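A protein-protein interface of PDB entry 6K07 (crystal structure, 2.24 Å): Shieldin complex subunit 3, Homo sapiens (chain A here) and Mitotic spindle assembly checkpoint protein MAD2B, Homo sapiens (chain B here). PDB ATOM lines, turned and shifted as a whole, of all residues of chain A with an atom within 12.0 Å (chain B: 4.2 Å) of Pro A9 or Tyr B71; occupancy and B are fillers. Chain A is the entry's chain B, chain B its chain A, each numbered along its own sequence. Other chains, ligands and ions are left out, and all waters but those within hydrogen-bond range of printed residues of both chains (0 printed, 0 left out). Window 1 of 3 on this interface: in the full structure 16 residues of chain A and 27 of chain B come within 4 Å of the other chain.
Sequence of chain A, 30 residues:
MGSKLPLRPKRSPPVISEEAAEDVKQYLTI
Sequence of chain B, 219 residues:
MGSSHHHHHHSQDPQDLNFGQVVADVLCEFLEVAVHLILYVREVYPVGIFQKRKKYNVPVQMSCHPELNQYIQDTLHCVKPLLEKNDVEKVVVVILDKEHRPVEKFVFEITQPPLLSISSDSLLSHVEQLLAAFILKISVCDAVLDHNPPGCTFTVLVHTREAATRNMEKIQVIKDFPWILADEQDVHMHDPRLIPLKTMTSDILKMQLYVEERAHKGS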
ATOM      1  N   LEU A   5     -12.563  19.597  -3.803  1.00  0.00           N
ATOM      2  CA  LEU A   5     -11.915  18.296  -4.002  1.00  0.00           C
ATOM      3  C   LEU A   5     -11.105  18.250  -5.307  1.00  0.00           C
ATOM      4  O   LEU A   5     -11.632  18.496  -6.381  1.00  0.00           O
ATOM      5  CB  LEU A   5     -12.958  17.173  -3.985  1.00  0.00           C
ATOM      6  CG  LEU A   5     -12.571  15.905  -3.210  1.00  0.00           C
ATOM      7  CD1 LEU A   5     -12.058  16.272  -1.834  1.00  0.00           C
ATOM      8  CD2 LEU A   5     -13.749  14.966  -3.081  1.00  0.00           C
ATOM      9  N   PRO A   6      -9.831  17.909  -5.218  1.00  0.00           N
ATOM     10  CA  PRO A   6      -8.924  18.084  -6.355  1.00  0.00           C
ATOM     11  C   PRO A   6      -9.128  17.036  -7.450  1.00  0.00           C
ATOM     12  O   PRO A   6      -9.920  16.095  -7.341  1.00  0.00           O
ATOM     13  CB  PRO A   6      -7.535  17.950  -5.718  1.00  0.00           C
ATOM     14  CG  PRO A   6      -7.747  17.070  -4.548  1.00  0.00           C
ATOM     15  CD  PRO A   6      -9.140  17.374  -4.034  1.00  0.00           C
ATOM     16  N   LEU A   7      -8.385  17.243  -8.533  1.00  0.00           N
ATOM     17  CA  LEU A   7      -8.275  16.312  -9.636  1.00  0.00           C
ATOM     18  C   LEU A   7      -7.013  15.485  -9.477  1.00  0.00           C
ATOM     19  O   LEU A   7      -6.005  15.938  -8.915  1.00  0.00           O
ATOM     20  CB  LEU A   7      -8.213  17.036 -10.977  1.00  0.00           C
ATOM     21  CG  LEU A   7      -9.385  17.917 -11.386  1.00  0.00           C
ATOM     22  CD1 LEU A   7      -9.090  18.642 -12.696  1.00  0.00           C
ATOM     23  CD2 LEU A   7     -10.590  17.060 -11.524  1.00  0.00           C
ATOM     24  N   ARG A   8      -7.073  14.271 -10.001  1.00  0.00           N
ATOM     25  CA  ARG A   8      -5.925  13.383 -10.027  1.00  0.00           C
ATOM     26  C   ARG A   8      -5.972  12.600 -11.324  1.00  0.00           C
ATOM     27  O   ARG A   8      -7.016  12.529 -11.983  1.00  0.00           O
ATOM     28  CB  ARG A   8      -5.912  12.440  -8.815  1.00  0.00           C
ATOM     29  CG  ARG A   8      -7.081  11.502  -8.748  1.00  0.00           C
ATOM     30  CD  ARG A   8      -6.701  10.186  -8.092  1.00  0.00           C
ATOM     31  NE  ARG A   8      -7.788   9.214  -8.215  1.00  0.00           N
ATOM     32  CZ  ARG A   8      -7.700   7.934  -7.860  1.00  0.00           C
ATOM     33  NH1 ARG A   8      -6.564   7.469  -7.357  1.00  0.00           N
ATOM     34  NH2 ARG A   8      -8.746   7.122  -8.005  1.00  0.00           N
ATOM     35  N   PRO A   9      -4.854  12.027 -11.735  1.00  0.00           N
ATOM     36  CA  PRO A   9      -4.893  11.141 -12.894  1.00  0.00           C
ATOM     37  C   PRO A   9      -5.712   9.910 -12.569  1.00  0.00           C
ATOM     38  O   PRO A   9      -5.652   9.390 -11.455  1.00  0.00           O
ATOM     39  CB  PRO A   9      -3.413  10.805 -13.138  1.00  0.00           C
ATOM     40  CG  PRO A   9      -2.646  11.905 -12.418  1.00  0.00           C
ATOM     41  CD  PRO A   9      -3.483  12.213 -11.223  1.00  0.00           C
ATOM     42  N   LYS A  10      -6.497   9.458 -13.550  1.00  0.00           N
ATOM     43  CA  LYS A  10      -7.186   8.182 -13.405  1.00  0.00           C
ATOM     44  C   LYS A  10      -6.203   7.028 -13.450  1.00  0.00           C
ATOM     45  O   LYS A  10      -6.458   5.973 -12.859  1.00  0.00           O
ATOM     46  CB  LYS A  10      -8.244   8.006 -14.495  1.00  0.00           C
ATOM     47  CG  LYS A  10      -9.190   6.816 -14.272  1.00  0.00           C
ATOM     48  CD  LYS A  10     -10.502   6.957 -15.060  1.00  0.00           C
ATOM     49  CE  LYS A  10     -11.184   5.594 -15.381  1.00  0.00           C
ATOM     50  NZ  LYS A  10     -10.865   5.016 -16.741  1.00  0.00           N
ATOM     51  N   ARG A  11      -5.084   7.204 -14.140  1.00  0.00           N
ATOM     52  CA  ARG A  11      -4.099   6.145 -14.276  1.00  0.00           C
ATOM     53  C   ARG A  11      -3.145   6.191 -13.091  1.00  0.00           C
ATOM     54  O   ARG A  11      -2.687   7.262 -12.683  1.00  0.00           O
ATOM     55  CB  ARG A  11      -3.322   6.277 -15.591  1.00  0.00           C
ATOM     56  N   SER A  12      -2.879   5.039 -12.532  1.00  0.00           N
ATOM     57  CA  SER A  12      -1.950   4.898 -11.424  1.00  0.00           C
ATOM     58  C   SER A  12      -0.520   4.854 -11.951  1.00  0.00           C
ATOM     59  O   SER A  12      -0.289   4.445 -13.089  1.00  0.00           O
ATOM     60  CB  SER A  12      -2.242   3.623 -10.636  1.00  0.00           C
ATOM     61  OG  SER A  12      -2.324   2.490 -11.507  1.00  0.00           O
ATOM     62  N   PRO A  13       0.452   5.303 -11.162  1.00  0.00           N
ATOM     63  CA  PRO A  13       1.856   5.187 -11.568  1.00  0.00           C
ATOM     64  C   PRO A  13       2.264   3.729 -11.627  1.00  0.00           C
ATOM     65  O   PRO A  13       1.599   2.884 -11.017  1.00  0.00           O
ATOM     66  CB  PRO A  13       2.605   5.929 -10.454  1.00  0.00           C
ATOM     67  CG  PRO A  13       1.713   5.789  -9.299  1.00  0.00           C
ATOM     68  CD  PRO A  13       0.336   5.984  -9.867  1.00  0.00           C
ATOM     69  N   PRO A  14       3.354   3.397 -12.326  1.00  0.00           N
ATOM     70  CA  PRO A  14       3.691   1.981 -12.518  1.00  0.00           C
ATOM     71  C   PRO A  14       4.147   1.330 -11.220  1.00  0.00           C
ATOM     72  O   PRO A  14       4.616   1.996 -10.292  1.00  0.00           O
ATOM     73  CB  PRO A  14       4.824   2.016 -13.558  1.00  0.00           C
ATOM     74  CG  PRO A  14       5.459   3.346 -13.373  1.00  0.00           C
ATOM     75  CD  PRO A  14       4.365   4.293 -12.915  1.00  0.00           C
ATOM     76  N   VAL A  15       3.972   0.012 -11.162  1.00  0.00           N
ATOM     77  CA  VAL A  15       4.573  -0.841 -10.141  1.00  0.00           C
ATOM     78  C   VAL A  15       5.908  -1.333 -10.680  1.00  0.00           C
ATOM     79  O   VAL A  15       6.006  -1.715 -11.849  1.00  0.00           O
ATOM     80  CB  VAL A  15       3.645  -2.020  -9.801  1.00  0.00           C
ATOM     81  CG1 VAL A  15       4.299  -2.948  -8.808  1.00  0.00           C
ATOM     82  CG2 VAL A  15       2.319  -1.516  -9.254  1.00  0.00           C
ATOM     83  N   ILE A  16       6.950  -1.286  -9.857  1.00  0.00           N
ATOM     84  CA  ILE A  16       8.300  -1.596 -10.311  1.00  0.00           C
ATOM     85  C   ILE A  16       8.821  -2.748  -9.467  1.00  0.00           C
ATOM     86  O   ILE A  16       9.089  -2.577  -8.269  1.00  0.00           O
ATOM     87  CB  ILE A  16       9.235  -0.389 -10.231  1.00  0.00           C
ATOM     88  CG1 ILE A  16       8.658   0.784 -11.019  1.00  0.00           C
ATOM     89  CG2 ILE A  16      10.634  -0.734 -10.774  1.00  0.00           C
ATOM     90  CD1 ILE A  16       9.629   1.943 -11.136  1.00  0.00           C
ATOM     91  N   GLU B  67       8.968   3.874 -17.810  1.00  0.00           N
ATOM     92  CA  GLU B  67       7.559   4.211 -17.707  1.00  0.00           C
ATOM     93  C   GLU B  67       7.242   5.025 -16.481  1.00  0.00           C
ATOM     94  O   GLU B  67       6.305   5.837 -16.544  1.00  0.00           O
ATOM     95  CB  GLU B  67       6.628   2.993 -17.769  1.00  0.00           C
ATOM     96  CG  GLU B  67       6.188   2.731 -19.231  1.00  0.00           C
ATOM     97  CD  GLU B  67       5.346   3.874 -19.822  1.00  0.00           C
ATOM     98  OE1 GLU B  67       4.662   4.610 -19.051  1.00  0.00           O
ATOM     99  OE2 GLU B  67       5.448   4.052 -21.073  1.00  0.00           O
ATOM    100  N   LEU B  68       7.992   4.882 -15.377  1.00  0.00           N
ATOM    101  CA  LEU B  68       7.784   5.842 -14.303  1.00  0.00           C
ATOM    102  C   LEU B  68       8.054   7.244 -14.818  1.00  0.00           C
ATOM    103  O   LEU B  68       7.269   8.170 -14.593  1.00  0.00           O
ATOM    104  CB  LEU B  68       8.661   5.533 -13.094  1.00  0.00           C
ATOM    105  CG  LEU B  68       8.557   6.632 -12.034  1.00  0.00           C
ATOM    106  CD1 LEU B  68       7.107   6.764 -11.679  1.00  0.00           C
ATOM    107  CD2 LEU B  68       9.405   6.411 -10.759  1.00  0.00           C
ATOM    108  N   ASN B  69       9.151   7.404 -15.544  1.00  0.00           N
ATOM    109  CA  ASN B  69       9.491   8.703 -16.108  1.00  0.00           C
ATOM    110  C   ASN B  69       8.415   9.197 -17.063  1.00  0.00           C
ATOM    111  O   ASN B  69       8.082  10.380 -17.050  1.00  0.00           O
ATOM    112  CB  ASN B  69      10.832   8.625 -16.831  1.00  0.00           C
ATOM    113  CG  ASN B  69      11.992   8.363 -15.885  1.00  0.00           C
ATOM    114  OD1 ASN B  69      11.832   8.352 -14.658  1.00  0.00           O
ATOM    115  ND2 ASN B  69      13.171   8.137 -16.452  1.00  0.00           N
ATOM    116  N   GLN B  70       7.884   8.322 -17.924  1.00  0.00           N
ATOM    117  CA  GLN B  70       6.806   8.752 -18.818  1.00  0.00           C
ATOM    118  C   GLN B  70       5.558   9.148 -18.033  1.00  0.00           C
ATOM    119  O   GLN B  70       4.828  10.060 -18.429  1.00  0.00           O
ATOM    120  CB  GLN B  70       6.459   7.655 -19.823  1.00  0.00           C
ATOM    121  CG  GLN B  70       5.552   8.141 -20.972  1.00  0.00           C
ATOM    122  CD  GLN B  70       6.156   9.289 -21.780  1.00  0.00           C
ATOM    123  OE1 GLN B  70       7.213   9.160 -22.399  1.00  0.00           O
ATOM    124  NE2 GLN B  70       5.487  10.421 -21.766  1.00  0.00           N
ATOM    125  N   TYR B  71       5.291   8.477 -16.919  1.00  0.00           N
ATOM    126  CA  TYR B  71       4.077   8.788 -16.187  1.00  0.00           C
ATOM    127  C   TYR B  71       4.167  10.169 -15.544  1.00  0.00           C
ATOM    128  O   TYR B  71       3.179  10.922 -15.519  1.00  0.00           O
ATOM    129  CB  TYR B  71       3.830   7.690 -15.152  1.00  0.00           C
ATOM    130  CG  TYR B  71       2.623   7.902 -14.263  1.00  0.00           C
ATOM    131  CD1 TYR B  71       2.736   8.595 -13.066  1.00  0.00           C
ATOM    132  CD2 TYR B  71       1.373   7.401 -14.607  1.00  0.00           C
ATOM    133  CE1 TYR B  71       1.652   8.793 -12.244  1.00  0.00           C
ATOM    134  CE2 TYR B  71       0.280   7.595 -13.774  1.00  0.00           C
ATOM    135  CZ  TYR B  71       0.434   8.288 -12.603  1.00  0.00           C
ATOM    136  OH  TYR B  71      -0.632   8.495 -11.754  1.00  0.00           O
ATOM    137  N   ILE B  72       5.338  10.518 -15.004  1.00  0.00           N
ATOM    138  CA  ILE B  72       5.513  11.833 -14.383  1.00  0.00           C
ATOM    139  C   ILE B  72       5.437  12.946 -15.428  1.00  0.00           C
ATOM    140  O   ILE B  72       4.912  14.036 -15.159  1.00  0.00           O
ATOM    141  CB  ILE B  72       6.840  11.874 -13.608  1.00  0.00           C
ATOM    142  CG1 ILE B  72       6.792  10.839 -12.495  1.00  0.00           C
ATOM    143  CG2 ILE B  72       7.164  13.306 -13.099  1.00  0.00           C
ATOM    144  CD1 ILE B  72       8.103  10.626 -11.853  1.00  0.00           C
ATOM    145  N   GLN B  73       5.962  12.705 -16.626  1.00  0.00           N
ATOM    146  CA  GLN B  73       5.866  13.713 -17.684  1.00  0.00           C
ATOM    147  C   GLN B  73       4.428  13.910 -18.149  1.00  0.00           C
ATOM    148  O   GLN B  73       3.986  15.045 -18.355  1.00  0.00           O
ATOM    149  CB  GLN B  73       6.737  13.318 -18.876  1.00  0.00           C
ATOM    150  CG  GLN B  73       8.184  13.250 -18.516  1.00  0.00           C
ATOM    151  CD  GLN B  73       9.080  13.144 -19.717  1.00  0.00           C
ATOM    152  OE1 GLN B  73       8.624  12.926 -20.851  1.00  0.00           O
ATOM    153  NE2 GLN B  73      10.377  13.277 -19.474  1.00  0.00           N
ATOM    154  N   ASP B  74       3.700  12.816 -18.384  1.00  0.00           N
ATOM    155  CA  ASP B  74       2.311  12.939 -18.781  1.00  0.00           C
ATOM    156  C   ASP B  74       1.520  13.697 -17.724  1.00  0.00           C
ATOM    157  O   ASP B  74       0.669  14.536 -18.049  1.00  0.00           O
ATOM    158  CB  ASP B  74       1.720  11.553 -19.014  1.00  0.00           C
ATOM    159  CG  ASP B  74       2.296  10.850 -20.253  1.00  0.00           C
ATOM    160  OD1 ASP B  74       2.920  11.531 -21.102  1.00  0.00           O
ATOM    161  OD2 ASP B  74       2.087   9.613 -20.380  1.00  0.00           O
ATOM    162  N   THR B  75       1.785  13.418 -16.444  1.00  0.00           N
ATOM    163  CA  THR B  75       1.072  14.133 -15.402  1.00  0.00           C
ATOM    164  C   THR B  75       1.327  15.621 -15.518  1.00  0.00           C
ATOM    165  O   THR B  75       0.387  16.414 -15.630  1.00  0.00           O
ATOM    166  CB  THR B  75       1.488  13.614 -14.032  1.00  0.00           C
ATOM    167  OG1 THR B  75       1.200  12.206 -13.953  1.00  0.00           O
ATOM    168  CG2 THR B  75       0.706  14.321 -12.963  1.00  0.00           C
ATOM    169  N   THR B 155       0.548   9.503  -5.762  1.00  0.00           N
ATOM    170  CA  THR B 155      -0.235  10.123  -6.824  1.00  0.00           C
ATOM    171  C   THR B 155      -0.082  11.634  -6.725  1.00  0.00           C
ATOM    172  O   THR B 155       0.588  12.160  -5.828  1.00  0.00           O
ATOM    173  CB  THR B 155      -1.704   9.736  -6.764  1.00  0.00           C
ATOM    174  OG1 THR B 155      -2.439  10.635  -7.604  1.00  0.00           O
ATOM    175  CG2 THR B 155      -2.214   9.822  -5.356  1.00  0.00           C
ATOM    176  N   VAL B 156      -0.703  12.332  -7.667  1.00  0.00           N
ATOM    177  CA  VAL B 156      -0.566  13.774  -7.781  1.00  0.00           C
ATOM    178  C   VAL B 156      -1.960  14.374  -7.808  1.00  0.00           C
ATOM    179  O   VAL B 156      -2.814  13.958  -8.603  1.00  0.00           O
ATOM    180  CB  VAL B 156       0.245  14.188  -9.022  1.00  0.00           C
ATOM    181  CG1 VAL B 156       0.460  15.693  -9.038  1.00  0.00           C
ATOM    182  CG2 VAL B 156       1.582  13.490  -9.026  1.00  0.00           C
ATOM    183  N   PHE B 177      -4.524   9.258 -21.100  1.00  0.00           N
ATOM    184  CA  PHE B 177      -4.134   9.621 -19.741  1.00  0.00           C
ATOM    185  C   PHE B 177      -5.243  10.438 -19.085  1.00  0.00           C
ATOM    186  O   PHE B 177      -5.098  11.648 -18.865  1.00  0.00           O
ATOM    187  CB  PHE B 177      -2.814  10.394 -19.762  1.00  0.00           C
ATOM    188  CG  PHE B 177      -2.096  10.367 -18.467  1.00  0.00           C
ATOM    189  CD1 PHE B 177      -1.331   9.274 -18.101  1.00  0.00           C
ATOM    190  CD2 PHE B 177      -2.222  11.418 -17.583  1.00  0.00           C
ATOM    191  CE1 PHE B 177      -0.685   9.235 -16.871  1.00  0.00           C
ATOM    192  CE2 PHE B 177      -1.566  11.379 -16.363  1.00  0.00           C
ATOM    193  CZ  PHE B 177      -0.793  10.283 -16.017  1.00  0.00           C
ATOM    194  N   PRO B 178      -6.369   9.800 -18.758  1.00  0.00           N
ATOM    195  CA  PRO B 178      -7.483  10.543 -18.163  1.00  0.00           C
ATOM    196  C   PRO B 178      -7.196  11.065 -16.758  1.00  0.00           C
ATOM    197  O   PRO B 178      -6.365  10.540 -16.013  1.00  0.00           O
ATOM    198  CB  PRO B 178      -8.624   9.519 -18.156  1.00  0.00           C
ATOM    199  CG  PRO B 178      -7.962   8.189 -18.273  1.00  0.00           C
ATOM    200  CD  PRO B 178      -6.755   8.418 -19.098  1.00  0.00           C
ATOM    201  N   TRP B 179      -7.893  12.149 -16.430  1.00  0.00           N
ATOM    202  CA  TRP B 179      -7.963  12.746 -15.107  1.00  0.00           C
ATOM    203  C   TRP B 179      -9.377  12.586 -14.564  1.00  0.00           C
ATOM    204  O   TRP B 179     -10.341  12.543 -15.326  1.00  0.00           O
ATOM    205  CB  TRP B 179      -7.613  14.230 -15.160  1.00  0.00           C
ATOM    206  CG  TRP B 179      -6.181  14.451 -15.387  1.00  0.00           C
ATOM    207  CD1 TRP B 179      -5.479  14.189 -16.534  1.00  0.00           C
ATOM    208  CD2 TRP B 179      -5.235  14.985 -14.447  1.00  0.00           C
ATOM    209  NE1 TRP B 179      -4.157  14.531 -16.356  1.00  0.00           N
ATOM    210  CE2 TRP B 179      -3.987  15.013 -15.083  1.00  0.00           C
ATOM    211  CE3 TRP B 179      -5.331  15.444 -13.134  1.00  0.00           C
ATOM    212  CZ2 TRP B 179      -2.842  15.473 -14.446  1.00  0.00           C
ATOM    213  CZ3 TRP B 179      -4.200  15.908 -12.510  1.00  0.00           C
ATOM    214  CH2 TRP B 179      -2.967  15.916 -13.162  1.00  0.00           C
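The backbone carbonyl oxygen (O) of Arg A11 is in hydrogen-bond range of the side-chain hydroxyl (OH) of Tyr B71. The backbone nitrogen (N) of Pro A13 sits close to the side-chain hydroxyl (OH) of Tyr B71. The backbone carbonyl oxygen of Pro B178 lies within hydrogen-bond range of the backbone NH of Lys A10.
The backbone carbonyl oxygen of Tyr B71 lies within hydrogen-bond range of the side-chain hydroxyl of Thr B75 (2.8 Å).
Trp B179 touches Leu A7. Arg A8 touches Val B156 (CB to O, 3.5 Å). O of Arg A8 touches CA of Trp B179 (3.3 Å). CD of Pro A9 touches O of Val B156, 3.2 Å away. Phe B177 touches Pro A9 (CE2 to CB, 3.8 Å). Pro B178 touches Pro A9 (O to CA, 3.5 Å). Pro A9 touches Trp B179. Ser A12 touches Tyr B71. Pro A14 touches Glu B67 (CG to C, 3.96 Å). Pro A14 touches Leu B68.
Printed residues of chain B within 4 Å of Leu A7: Val B156 and Trp B179. Printed residues of chain B within 4 Å of Arg A8: Val B156 (3.5 Å) and Trp B179 (3.3 Å). Of chain B, only Tyr B71, Val B156, Phe B177, Pro B178 and Trp B179 come within 4 Å of Pro A9. Printed residues of chain B within 4 Å of Lys A10: Pro B178 (2.7 Å) and Trp B179 (3.9 Å). Of the printed residues of chain B, Pro A14 touches Glu B67 (3.96 Å) and Leu B68 (3.5 Å). Of chain A, only Pro A14 (3.96 Å) comes within 4 Å of Glu B67. Of chain A, only Pro A14 (3.5 Å) comes within 4 Å of Leu B68. Asn B69 touches none of the printed residues of chain A. Gln B70 touches none of the printed residues of chain A. Of chain A, only Pro A9 (3.9 Å), Arg A11 (2.6 Å), Ser A12 (3.3 Å) and Pro A13 (3.3 Å) come within 4 Å of Tyr B71. No residue of chain A comes within 4 Å of Ile B72. No residue of chain A comes within 4 Å of Gln B73. No residue of chain A comes within 4 Å of Asp B74. No residue of chain A comes within 4 Å of Thr B155. Val B156 touches three residues of chain A. Of chain A, only Pro A9 (3.5 Å) and Lys A10 (2.7 Å) come within 4 Å of Pro B178. Trp B179 touches just these residues of chain A: Leu A7 (3.9 Å), Arg A8 (3.3 Å), Pro A9 (3.7 Å) and Lys A10 (3.9 Å). The nearest residue of chain B that does not touch Pro A9 is Thr B155 (4.1 Å). The nearest printed residue of chain B that does not touch Leu A7 is Thr B155 (6.5 Å).
Printed residues of chain B that touch a printed residue of chain A: Glu B67, Leu B68, Tyr B71, Val B156, Phe B177, Pro B178 and Trp B179. Along chain B the printed residues that touch a printed residue of chain A span positions 67 to 179. Along chain A the printed residues that touch a printed residue of chain B span positions 7 to 14.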
